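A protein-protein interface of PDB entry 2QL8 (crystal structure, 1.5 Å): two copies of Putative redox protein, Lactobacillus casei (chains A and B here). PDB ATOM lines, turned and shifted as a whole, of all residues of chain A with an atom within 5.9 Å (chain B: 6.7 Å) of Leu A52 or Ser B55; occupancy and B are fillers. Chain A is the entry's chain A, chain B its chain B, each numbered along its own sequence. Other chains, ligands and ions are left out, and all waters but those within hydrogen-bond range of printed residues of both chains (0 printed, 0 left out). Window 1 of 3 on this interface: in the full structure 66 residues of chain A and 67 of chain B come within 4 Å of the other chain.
Leu A52 touches just these residues of chain B: Ser B55 and Leu B126. Printed residues of chain B within 4 Å of Gly A53: Ala B16. Of the printed residues of chain A, Ala B16 touches Gly A53, Leu A54, Ser A57 and Val A81. Of the printed residues of chain A, Ser B55 touches Pro A48, Leu A51 and Leu A52. Printed residues of chain A within 4 Å of Cys B59: Pro A48. The nearest printed residue of chain B that does not touch Gly A53 is Ser B55 (6.2 Å).
N of Val A81 is in hydrogen-bond range of O of Ala B16 (2.8 Å). The backbone carbonyl oxygen of Pro A48 is in hydrogen-bond range of the side-chain hydroxyl of Ser B55, at 2.8 Å.
The backbone carbonyl oxygen (O) of Leu A54 sits at hydrogen-bond distance from the side-chain hydroxyl (OG) of Ser A57, at 3.3 Å. The backbone carbonyl oxygen (O) of Leu B54 is in hydrogen-bond range of the side-chain hydroxyl (OG) of Ser B57 (3.3 Å). The backbone carbonyl oxygen (O) of Gly A53 is in hydrogen-bond range of the side-chain hydroxyl (OG) of Ser A57, at 2.8 Å. SG of Cys B59 is in hydrogen-bond range of SG of Cys B121. The side-chain sulfur (SG) of Cys B121 lies close to the backbone NH (N) of Val B123 (3.6 Å). O of Leu B54 sits at hydrogen-bond distance from OG1 of Thr B58 (2.8 Å).
Leu A51 touches its own counterpart, Leu B51. Leu A51 touches Leu B54, and with the chains exchanged Leu A54 touches Leu B51. Leu A51 touches Ser B55, and with the chains exchanged Ser A55 touches Leu B51. Leu A52 touches Ser B55, and with the chains exchanged Ser A55 touches Leu B52. Positions printed for both chains: 50, 51, 52, 53, 54, 55, 56, 57, 81, 123 and 127.
Of the 17 printed residues of chain B, 9 touch a printed residue of chain A. Printed residues of chain A that touch a printed residue of chain B: Pro A48, Leu A51, Leu A52, Gly A53, Leu A54, Ser A55, Ser A57, Val A81, Phe A94 and Leu A127. Hydrophobic or aromatic side chains of chain A that line the printed part of chain B: Pro A48, Leu A51, Leu A52, Leu A54, Phe A94 and Leu A127. Among the printed residues, 18 pairs touch across the chains. Among the printed residues, no Asp or Glu carboxylate lies within 4 Å of a Lys or Arg side-chain nitrogen of the other chain.
Among the printed residues, pairs that only touch across the chains: Gly A53 with Ala B16 (3.2 Å), Leu A54 with Ala B16 (3.4 Å), Phe A94 with Val B123 (3.5 Å), Leu A52 with Leu B126 (3.5 Å), Phe A94 with Leu B126 (3.5 Å), Pro A48 with Cys B59 (3.6 Å), Pro A48 with Thr B58 (3.6 Å), Ser A55 with Leu B52 (3.6 Å), Leu A52 with Ser B55 (3.6 Å), Leu A51 with Ser B55 (3.7 Å), Ser A55 with Leu B51 (3.7 Å), Leu A54 with Leu B51 (3.8 Å), Leu A51 with Leu B54 (3.8 Å), Leu A127 with Leu B126 (3.9 Å), Leu A51 with Leu B51 (3.9 Å) and Ser A57 with Ala B16 (3.96 Å).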
ATOM      1  N   ASN A  47     -20.613   5.830  -7.521  1.00  0.00           N
ATOM      2  CA  ASN A  47     -19.921   7.092  -7.299  1.00  0.00           C
ATOM      3  C   ASN A  47     -20.285   7.634  -5.926  1.00  0.00           C
ATOM      4  O   ASN A  47     -21.167   7.071  -5.246  1.00  0.00           O
ATOM      5  CB  ASN A  47     -20.274   8.090  -8.437  1.00  0.00           C
ATOM      6  CG  ASN A  47     -21.781   8.252  -8.624  1.00  0.00           C
ATOM      7  OD1 ASN A  47     -22.468   8.644  -7.673  1.00  0.00           O
ATOM      8  ND2 ASN A  47     -22.300   7.950  -9.844  1.00  0.00           N
ATOM      9  N   PRO A  48     -19.555   8.647  -5.454  1.00  0.00           N
ATOM     10  CA  PRO A  48     -19.841   9.169  -4.104  1.00  0.00           C
ATOM     11  C   PRO A  48     -21.256   9.685  -3.881  1.00  0.00           C
ATOM     12  O   PRO A  48     -21.786   9.578  -2.761  1.00  0.00           O
ATOM     13  CB  PRO A  48     -18.823  10.283  -3.946  1.00  0.00           C
ATOM     14  CG  PRO A  48     -17.676   9.865  -4.827  1.00  0.00           C
ATOM     15  CD  PRO A  48     -18.359   9.304  -6.049  1.00  0.00           C
ATOM     16  N   GLU A  49     -21.860  10.231  -4.933  1.00  0.00           N
ATOM     17  CA  GLU A  49     -23.206  10.771  -4.876  1.00  0.00           C
ATOM     18  C   GLU A  49     -24.198   9.648  -4.574  1.00  0.00           C
ATOM     19  O   GLU A  49     -25.021   9.719  -3.644  1.00  0.00           O
ATOM     20  CB  GLU A  49     -23.551  11.430  -6.212  1.00  0.00           C
ATOM     21  CG  GLU A  49     -22.767  12.734  -6.518  1.00  0.00           C
ATOM     22  CD  GLU A  49     -21.440  12.506  -7.302  1.00  0.00           C
ATOM     23  OE1 GLU A  49     -20.899  11.359  -7.306  1.00  0.00           O
ATOM     24  OE2 GLU A  49     -20.967  13.495  -7.922  1.00  0.00           O
ATOM     25  N   GLN A  50     -24.090   8.567  -5.342  1.00  0.00           N
ATOM     26  CA  GLN A  50     -24.934   7.394  -5.147  1.00  0.00           C
ATOM     27  C   GLN A  50     -24.710   6.770  -3.753  1.00  0.00           C
ATOM     28  O   GLN A  50     -25.664   6.387  -3.050  1.00  0.00           O
ATOM     29  CB  GLN A  50     -24.696   6.346  -6.222  1.00  0.00           C
ATOM     30  CG  GLN A  50     -25.238   6.746  -7.611  1.00  0.00           C
ATOM     31  CD  GLN A  50     -25.055   5.665  -8.659  1.00  0.00           C
ATOM     32  OE1 GLN A  50     -24.508   4.592  -8.383  1.00  0.00           O
ATOM     33  NE2 GLN A  50     -25.534   5.950  -9.890  1.00  0.00           N
ATOM     34  N   LEU A  51     -23.443   6.598  -3.393  1.00  0.00           N
ATOM     35  CA  LEU A  51     -23.081   5.949  -2.140  1.00  0.00           C
ATOM     36  C   LEU A  51     -23.610   6.754  -0.951  1.00  0.00           C
ATOM     37  O   LEU A  51     -24.135   6.172   0.019  1.00  0.00           O
ATOM     38  CB  LEU A  51     -21.576   5.697  -2.072  1.00  0.00           C
ATOM     39  CG  LEU A  51     -21.073   4.586  -2.999  1.00  0.00           C
ATOM     40  CD1 LEU A  51     -19.538   4.767  -3.247  1.00  0.00           C
ATOM     41  CD2 LEU A  51     -21.437   3.209  -2.441  1.00  0.00           C
ATOM     42  N   LEU A  52     -23.500   8.068  -1.012  1.00  0.00           N
ATOM     43  CA  LEU A  52     -24.092   8.954  -0.007  1.00  0.00           C
ATOM     44  C   LEU A  52     -25.602   8.831   0.089  1.00  0.00           C
ATOM     45  O   LEU A  52     -26.177   8.724   1.165  1.00  0.00           O
ATOM     46  CB  LEU A  52     -23.680  10.392  -0.219  1.00  0.00           C
ATOM     47  CG  LEU A  52     -24.214  11.465   0.738  1.00  0.00           C
ATOM     48  CD1 LEU A  52     -23.792  11.109   2.194  1.00  0.00           C
ATOM     49  CD2 LEU A  52     -23.789  12.894   0.386  1.00  0.00           C
ATOM     50  N   GLY A  53     -26.266   8.808  -1.058  1.00  0.00           N
ATOM     51  CA  GLY A  53     -27.700   8.595  -1.068  1.00  0.00           C
ATOM     52  C   GLY A  53     -28.118   7.249  -0.470  1.00  0.00           C
ATOM     53  O   GLY A  53     -29.107   7.154   0.272  1.00  0.00           O
ATOM     54  N   LEU A  54     -27.389   6.195  -0.803  1.00  0.00           N
ATOM     55  CA  LEU A  54     -27.625   4.876  -0.222  1.00  0.00           C
ATOM     56  C   LEU A  54     -27.423   4.894   1.297  1.00  0.00           C
ATOM     57  O   LEU A  54     -28.206   4.302   2.047  1.00  0.00           O
ATOM     58  CB  LEU A  54     -26.738   3.792  -0.876  1.00  0.00           C
ATOM     59  CG  LEU A  54     -27.011   3.451  -2.362  1.00  0.00           C
ATOM     60  CD1 LEU A  54     -25.846   2.659  -3.000  1.00  0.00           C
ATOM     61  CD2 LEU A  54     -28.369   2.696  -2.502  1.00  0.00           C
ATOM     62  N   SER A  55     -26.376   5.574   1.739  1.00  0.00           N
ATOM     63  CA  SER A  55     -26.126   5.710   3.177  1.00  0.00           C
ATOM     64  C   SER A  55     -27.280   6.428   3.903  1.00  0.00           C
ATOM     65  O   SER A  55     -27.833   5.921   4.916  1.00  0.00           O
ATOM     66  CB  SER A  55     -24.811   6.459   3.438  1.00  0.00           C
ATOM     67  OG  SER A  55     -24.594   6.656   4.832  1.00  0.00           O
ATOM     68  N   LEU A  56     -27.626   7.619   3.432  1.00  0.00           N
ATOM     69  CA  LEU A  56     -28.658   8.439   4.089  1.00  0.00           C
ATOM     70  C   LEU A  56     -30.041   7.795   4.021  1.00  0.00           C
ATOM     71  O   LEU A  56     -30.767   7.775   5.004  1.00  0.00           O
ATOM     72  CB  LEU A  56     -28.678   9.846   3.515  1.00  0.00           C
ATOM     73  CG  LEU A  56     -29.707  10.818   4.113  1.00  0.00           C
ATOM     74  CD1 LEU A  56     -29.518  11.001   5.636  1.00  0.00           C
ATOM     75  CD2 LEU A  56     -29.683  12.143   3.374  1.00  0.00           C
ATOM     76  N   SER A  57     -30.424   7.311   2.847  1.00  0.00           N
ATOM     77  CA  SER A  57     -31.733   6.650   2.722  1.00  0.00           C
ATOM     78  C   SER A  57     -31.847   5.486   3.705  1.00  0.00           C
ATOM     79  O   SER A  57     -32.890   5.301   4.355  1.00  0.00           O
ATOM     80  CB  SER A  57     -32.002   6.224   1.255  1.00  0.00           C
ATOM     81  OG  SER A  57     -31.097   5.215   0.796  1.00  0.00           O
ATOM     82  N   VAL A  81     -33.619   9.539  -1.464  1.00  0.00           N
ATOM     83  CA  VAL A  81     -32.682  10.633  -1.344  1.00  0.00           C
ATOM     84  C   VAL A  81     -32.173  10.955  -2.742  1.00  0.00           C
ATOM     85  O   VAL A  81     -31.665  10.070  -3.442  1.00  0.00           O
ATOM     86  CB  VAL A  81     -31.499  10.279  -0.381  1.00  0.00           C
ATOM     87  CG1 VAL A  81     -30.408  11.354  -0.417  1.00  0.00           C
ATOM     88  CG2 VAL A  81     -32.031  10.027   1.052  1.00  0.00           C
ATOM     89  N   VAL A  83     -29.317  13.213  -4.760  1.00  0.00           N
ATOM     90  CA  VAL A  83     -28.041  13.901  -4.570  1.00  0.00           C
ATOM     91  C   VAL A  83     -27.656  14.524  -5.920  1.00  0.00           C
ATOM     92  O   VAL A  83     -27.696  13.836  -6.949  1.00  0.00           O
ATOM     93  CB  VAL A  83     -26.911  12.944  -4.085  1.00  0.00           C
ATOM     94  CG1 VAL A  83     -25.584  13.705  -3.881  1.00  0.00           C
ATOM     95  CG2 VAL A  83     -27.348  12.229  -2.794  1.00  0.00           C
ATOM     96  N   PHE A  94     -21.925  18.870  -3.296  1.00  0.00           N
ATOM     97  CA  PHE A  94     -23.096  18.020  -3.407  1.00  0.00           C
ATOM     98  C   PHE A  94     -24.273  18.703  -2.696  1.00  0.00           C
ATOM     99  O   PHE A  94     -24.107  19.329  -1.626  1.00  0.00           O
ATOM    100  CB  PHE A  94     -22.894  16.654  -2.749  1.00  0.00           C
ATOM    101  CG  PHE A  94     -21.912  15.745  -3.422  1.00  0.00           C
ATOM    102  CD1 PHE A  94     -21.284  16.045  -4.636  1.00  0.00           C
ATOM    103  CD2 PHE A  94     -21.592  14.551  -2.818  1.00  0.00           C
ATOM    104  CE1 PHE A  94     -20.397  15.164  -5.194  1.00  0.00           C
ATOM    105  CE2 PHE A  94     -20.654  13.681  -3.385  1.00  0.00           C
ATOM    106  CZ  PHE A  94     -20.058  14.021  -4.568  1.00  0.00           C
ATOM    107  N   VAL A  96     -28.170  17.564  -1.205  1.00  0.00           N
ATOM    108  CA  VAL A  96     -28.849  16.361  -0.764  1.00  0.00           C
ATOM    109  C   VAL A  96     -30.295  16.702  -0.350  1.00  0.00           C
ATOM    110  O   VAL A  96     -30.534  17.650   0.424  1.00  0.00           O
ATOM    111  CB  VAL A  96     -28.140  15.747   0.468  1.00  0.00           C
ATOM    112  CG1 VAL A  96     -28.877  14.465   0.936  1.00  0.00           C
ATOM    113  CG2 VAL A  96     -26.619  15.501   0.174  1.00  0.00           C
ATOM    114  N   VAL A 123     -26.769  10.164  10.015  1.00  0.00           N
ATOM    115  CA  VAL A 123     -26.254  10.775   8.777  1.00  0.00           C
ATOM    116  C   VAL A 123     -26.907  12.158   8.602  1.00  0.00           C
ATOM    117  O   VAL A 123     -26.259  13.117   8.213  1.00  0.00           O
ATOM    118  CB  VAL A 123     -26.404   9.864   7.536  1.00  0.00           C
ATOM    119  CG1 VAL A 123     -25.847  10.585   6.270  1.00  0.00           C
ATOM    120  CG2 VAL A 123     -25.697   8.492   7.754  1.00  0.00           C
ATOM    121  N   LEU A 127     -25.103  16.058   8.313  1.00  0.00           N
ATOM    122  CA  LEU A 127     -25.371  16.995   7.208  1.00  0.00           C
ATOM    123  C   LEU A 127     -26.114  18.257   7.641  1.00  0.00           C
ATOM    124  O   LEU A 127     -26.228  19.206   6.847  1.00  0.00           O
ATOM    125  CB  LEU A 127     -26.189  16.292   6.135  1.00  0.00           C
ATOM    126  CG  LEU A 127     -25.626  15.025   5.488  1.00  0.00           C
ATOM    127  CD1 LEU A 127     -26.615  14.353   4.492  1.00  0.00           C
ATOM    128  CD2 LEU A 127     -24.265  15.359   4.839  1.00  0.00           C
ATOM    129  N   ALA B  16     -31.441   7.506  -4.564  1.00  0.00           N
ATOM    130  CA  ALA B  16     -31.278   6.266  -3.825  1.00  0.00           C
ATOM    131  C   ALA B  16     -32.554   6.060  -3.018  1.00  0.00           C
ATOM    132  O   ALA B  16     -33.112   7.012  -2.480  1.00  0.00           O
ATOM    133  CB  ALA B  16     -30.102   6.343  -2.863  1.00  0.00           C
ATOM    134  N   GLN B  50     -20.731   1.931   6.606  1.00  0.00           N
ATOM    135  CA  GLN B  50     -19.959   1.454   5.463  1.00  0.00           C
ATOM    136  C   GLN B  50     -20.186   2.287   4.209  1.00  0.00           C
ATOM    137  O   GLN B  50     -19.232   2.671   3.494  1.00  0.00           O
ATOM    138  CB  GLN B  50     -20.265  -0.021   5.159  1.00  0.00           C
ATOM    139  CG  GLN B  50     -19.680  -0.974   6.220  1.00  0.00           C
ATOM    140  CD  GLN B  50     -19.916  -2.425   5.950  1.00  0.00           C
ATOM    141  OE1 GLN B  50     -20.524  -2.762   4.944  1.00  0.00           O
ATOM    142  NE2 GLN B  50     -19.487  -3.289   6.874  1.00  0.00           N
ATOM    143  N   LEU B  51     -21.461   2.542   3.906  1.00  0.00           N
ATOM    144  CA  LEU B  51     -21.798   3.279   2.675  1.00  0.00           C
ATOM    145  C   LEU B  51     -21.227   4.715   2.710  1.00  0.00           C
ATOM    146  O   LEU B  51     -20.727   5.211   1.690  1.00  0.00           O
ATOM    147  CB  LEU B  51     -23.298   3.242   2.436  1.00  0.00           C
ATOM    148  CG  LEU B  51     -23.869   1.860   2.047  1.00  0.00           C
ATOM    149  CD1 LEU B  51     -25.409   1.794   2.289  1.00  0.00           C
ATOM    150  CD2 LEU B  51     -23.516   1.567   0.561  1.00  0.00           C
ATOM    151  N   LEU B  52     -21.262   5.355   3.878  1.00  0.00           N
ATOM    152  CA  LEU B  52     -20.685   6.670   4.044  1.00  0.00           C
ATOM    153  C   LEU B  52     -19.164   6.629   3.865  1.00  0.00           C
ATOM    154  O   LEU B  52     -18.587   7.481   3.171  1.00  0.00           O
ATOM    155  CB  LEU B  52     -21.058   7.266   5.401  1.00  0.00           C
ATOM    156  CG  LEU B  52     -20.497   8.657   5.724  1.00  0.00           C
ATOM    157  CD1 LEU B  52     -20.899   9.707   4.681  1.00  0.00           C
ATOM    158  CD2 LEU B  52     -20.816   9.093   7.204  1.00  0.00           C
ATOM    159  N   GLY B  53     -18.533   5.607   4.463  1.00  0.00           N
ATOM    160  CA  GLY B  53     -17.118   5.433   4.252  1.00  0.00           C
ATOM    161  C   GLY B  53     -16.733   5.242   2.786  1.00  0.00           C
ATOM    162  O   GLY B  53     -15.723   5.766   2.332  1.00  0.00           O
ATOM    163  N   LEU B  54     -17.497   4.399   2.082  1.00  0.00           N
ATOM    164  CA  LEU B  54     -17.284   4.192   0.651  1.00  0.00           C
ATOM    165  C   LEU B  54     -17.419   5.502  -0.127  1.00  0.00           C
ATOM    166  O   LEU B  54     -16.641   5.796  -1.061  1.00  0.00           O
ATOM    167  CB  LEU B  54     -18.222   3.122   0.120  1.00  0.00           C
ATOM    168  CG  LEU B  54     -17.989   1.698   0.595  1.00  0.00           C
ATOM    169  CD1 LEU B  54     -19.194   0.782   0.258  1.00  0.00           C
ATOM    170  CD2 LEU B  54     -16.665   1.098   0.059  1.00  0.00           C
ATOM    171  N   SER B  55     -18.440   6.290   0.208  1.00  0.00           N
ATOM    172  CA  SER B  55     -18.660   7.584  -0.447  1.00  0.00           C
ATOM    173  C   SER B  55     -17.496   8.535  -0.241  1.00  0.00           C
ATOM    174  O   SER B  55     -16.951   9.099  -1.221  1.00  0.00           O
ATOM    175  CB  SER B  55     -19.963   8.213   0.042  1.00  0.00           C
ATOM    176  OG  SER B  55     -20.163   9.512  -0.496  1.00  0.00           O
ATOM    177  N   LEU B  56     -17.131   8.725   1.026  1.00  0.00           N
ATOM    178  CA  LEU B  56     -16.086   9.709   1.340  1.00  0.00           C
ATOM    179  C   LEU B  56     -14.708   9.268   0.842  1.00  0.00           C
ATOM    180  O   LEU B  56     -13.940  10.084   0.314  1.00  0.00           O
ATOM    181  CB  LEU B  56     -16.050  10.023   2.843  1.00  0.00           C
ATOM    182  CG  LEU B  56     -14.953  10.964   3.330  1.00  0.00           C
ATOM    183  CD1 LEU B  56     -15.109  12.330   2.642  1.00  0.00           C
ATOM    184  CD2 LEU B  56     -15.005  11.101   4.875  1.00  0.00           C
ATOM    185  N   SER B  57     -14.365   7.994   1.024  1.00  0.00           N
ATOM    186  CA  SER B  57     -13.050   7.506   0.564  1.00  0.00           C
ATOM    187  C   SER B  57     -12.922   7.684  -0.960  1.00  0.00           C
ATOM    188  O   SER B  57     -11.890   8.108  -1.467  1.00  0.00           O
ATOM    189  CB  SER B  57     -12.805   6.033   0.944  1.00  0.00           C
ATOM    190  OG  SER B  57     -13.751   5.139   0.397  1.00  0.00           O
ATOM    191  N   THR B  58     -14.015   7.400  -1.673  1.00  0.00           N
ATOM    192  CA  THR B  58     -14.032   7.528  -3.139  1.00  0.00           C
ATOM    193  C   THR B  58     -13.909   8.997  -3.559  1.00  0.00           C
ATOM    194  O   THR B  58     -13.167   9.355  -4.501  1.00  0.00           O
ATOM    195  CB  THR B  58     -15.267   6.869  -3.737  1.00  0.00           C
ATOM    196  OG1 THR B  58     -15.256   5.468  -3.429  1.00  0.00           O
ATOM    197  CG2 THR B  58     -15.389   7.075  -5.249  1.00  0.00           C
ATOM    198  N   CYS B  59     -14.639   9.870  -2.877  1.00  0.00           N
ATOM    199  CA  CYS B  59     -14.600  11.303  -3.193  1.00  0.00           C
ATOM    200  C   CYS B  59     -13.230  11.905  -2.889  1.00  0.00           C
ATOM    201  O   CYS B  59     -12.666  12.630  -3.705  1.00  0.00           O
ATOM    202  CB  CYS B  59     -15.718  12.021  -2.451  1.00  0.00           C
ATOM    203  SG  CYS B  59     -16.135  13.650  -3.103  1.00  0.00           S
ATOM    204  N   LEU B  60     -12.674  11.571  -1.727  1.00  0.00           N
ATOM    205  CA  LEU B  60     -11.359  12.061  -1.360  1.00  0.00           C
ATOM    206  C   LEU B  60     -10.309  11.566  -2.380  1.00  0.00           C
ATOM    207  O   LEU B  60      -9.415  12.303  -2.789  1.00  0.00           O
ATOM    208  CB  LEU B  60     -10.968  11.648   0.069  1.00  0.00           C
ATOM    209  CG  LEU B  60     -11.534  12.523   1.171  1.00  0.00           C
ATOM    210  CD1 LEU B  60     -11.381  11.769   2.555  1.00  0.00           C
ATOM    211  CD2 LEU B  60     -10.982  13.946   1.216  1.00  0.00           C
ATOM    212  N   VAL B  81     -11.226   5.529   5.179  1.00  0.00           N
ATOM    213  CA  VAL B  81     -12.155   6.246   6.064  1.00  0.00           C
ATOM    214  C   VAL B  81     -12.659   5.244   7.105  1.00  0.00           C
ATOM    215  O   VAL B  81     -13.151   4.167   6.770  1.00  0.00           O
ATOM    216  CB  VAL B  81     -13.325   6.860   5.287  1.00  0.00           C
ATOM    217  CG1 VAL B  81     -14.369   7.446   6.233  1.00  0.00           C
ATOM    218  CG2 VAL B  81     -12.764   7.900   4.311  1.00  0.00           C
ATOM    219  N   CYS B 121     -12.969  18.384  -1.582  1.00  0.00           N
ATOM    220  CA  CYS B 121     -13.815  17.204  -1.705  1.00  0.00           C
ATOM    221  C   CYS B 121     -15.260  17.513  -1.278  1.00  0.00           C
ATOM    222  O   CYS B 121     -15.483  17.948  -0.149  1.00  0.00           O
ATOM    223  CB  CYS B 121     -13.232  16.098  -0.793  1.00  0.00           C
ATOM    224  SG  CYS B 121     -14.341  14.710  -0.438  1.00  0.00           S
ATOM    225  N   VAL B 123     -17.805  15.668  -0.300  1.00  0.00           N
ATOM    226  CA  VAL B 123     -18.311  14.988   0.901  1.00  0.00           C
ATOM    227  C   VAL B 123     -17.622  15.580   2.140  1.00  0.00           C
ATOM    228  O   VAL B 123     -18.259  15.772   3.184  1.00  0.00           O
ATOM    229  CB  VAL B 123     -18.202  13.442   0.800  1.00  0.00           C
ATOM    230  CG1 VAL B 123     -18.797  12.785   2.077  1.00  0.00           C
ATOM    231  CG2 VAL B 123     -18.928  12.903  -0.453  1.00  0.00           C
ATOM    232  N   LEU B 126     -19.358  18.700   3.056  1.00  0.00           N
ATOM    233  CA  LEU B 126     -20.642  18.453   3.736  1.00  0.00           C
ATOM    234  C   LEU B 126     -20.448  18.178   5.221  1.00  0.00           C
ATOM    235  O   LEU B 126     -21.301  18.470   6.043  1.00  0.00           O
ATOM    236  CB  LEU B 126     -21.411  17.295   3.093  1.00  0.00           C
ATOM    237  CG  LEU B 126     -22.006  17.437   1.686  1.00  0.00           C
ATOM    238  CD1 LEU B 126     -22.587  16.105   1.216  1.00  0.00           C
ATOM    239  CD2 LEU B 126     -23.050  18.608   1.681  1.00  0.00           C
ATOM    240  N   LEU B 127     -19.343  17.508   5.534  1.00  0.00           N
ATOM    241  CA  LEU B 127     -19.066  17.060   6.917  1.00  0.00           C
ATOM    242  C   LEU B 127     -18.326  18.098   7.757  1.00  0.00           C
ATOM    243  O   LEU B 127     -18.221  17.926   8.981  1.00  0.00           O
ATOM    244  CB  LEU B 127     -18.269  15.742   6.904  1.00  0.00           C
ATOM    245  CG  LEU B 127     -18.928  14.523   6.265  1.00  0.00           C
ATOM    246  CD1 LEU B 127     -17.933  13.362   6.237  1.00  0.00           C
ATOM    247  CD2 LEU B 127     -20.259  14.130   6.969  1.00  0.00           C
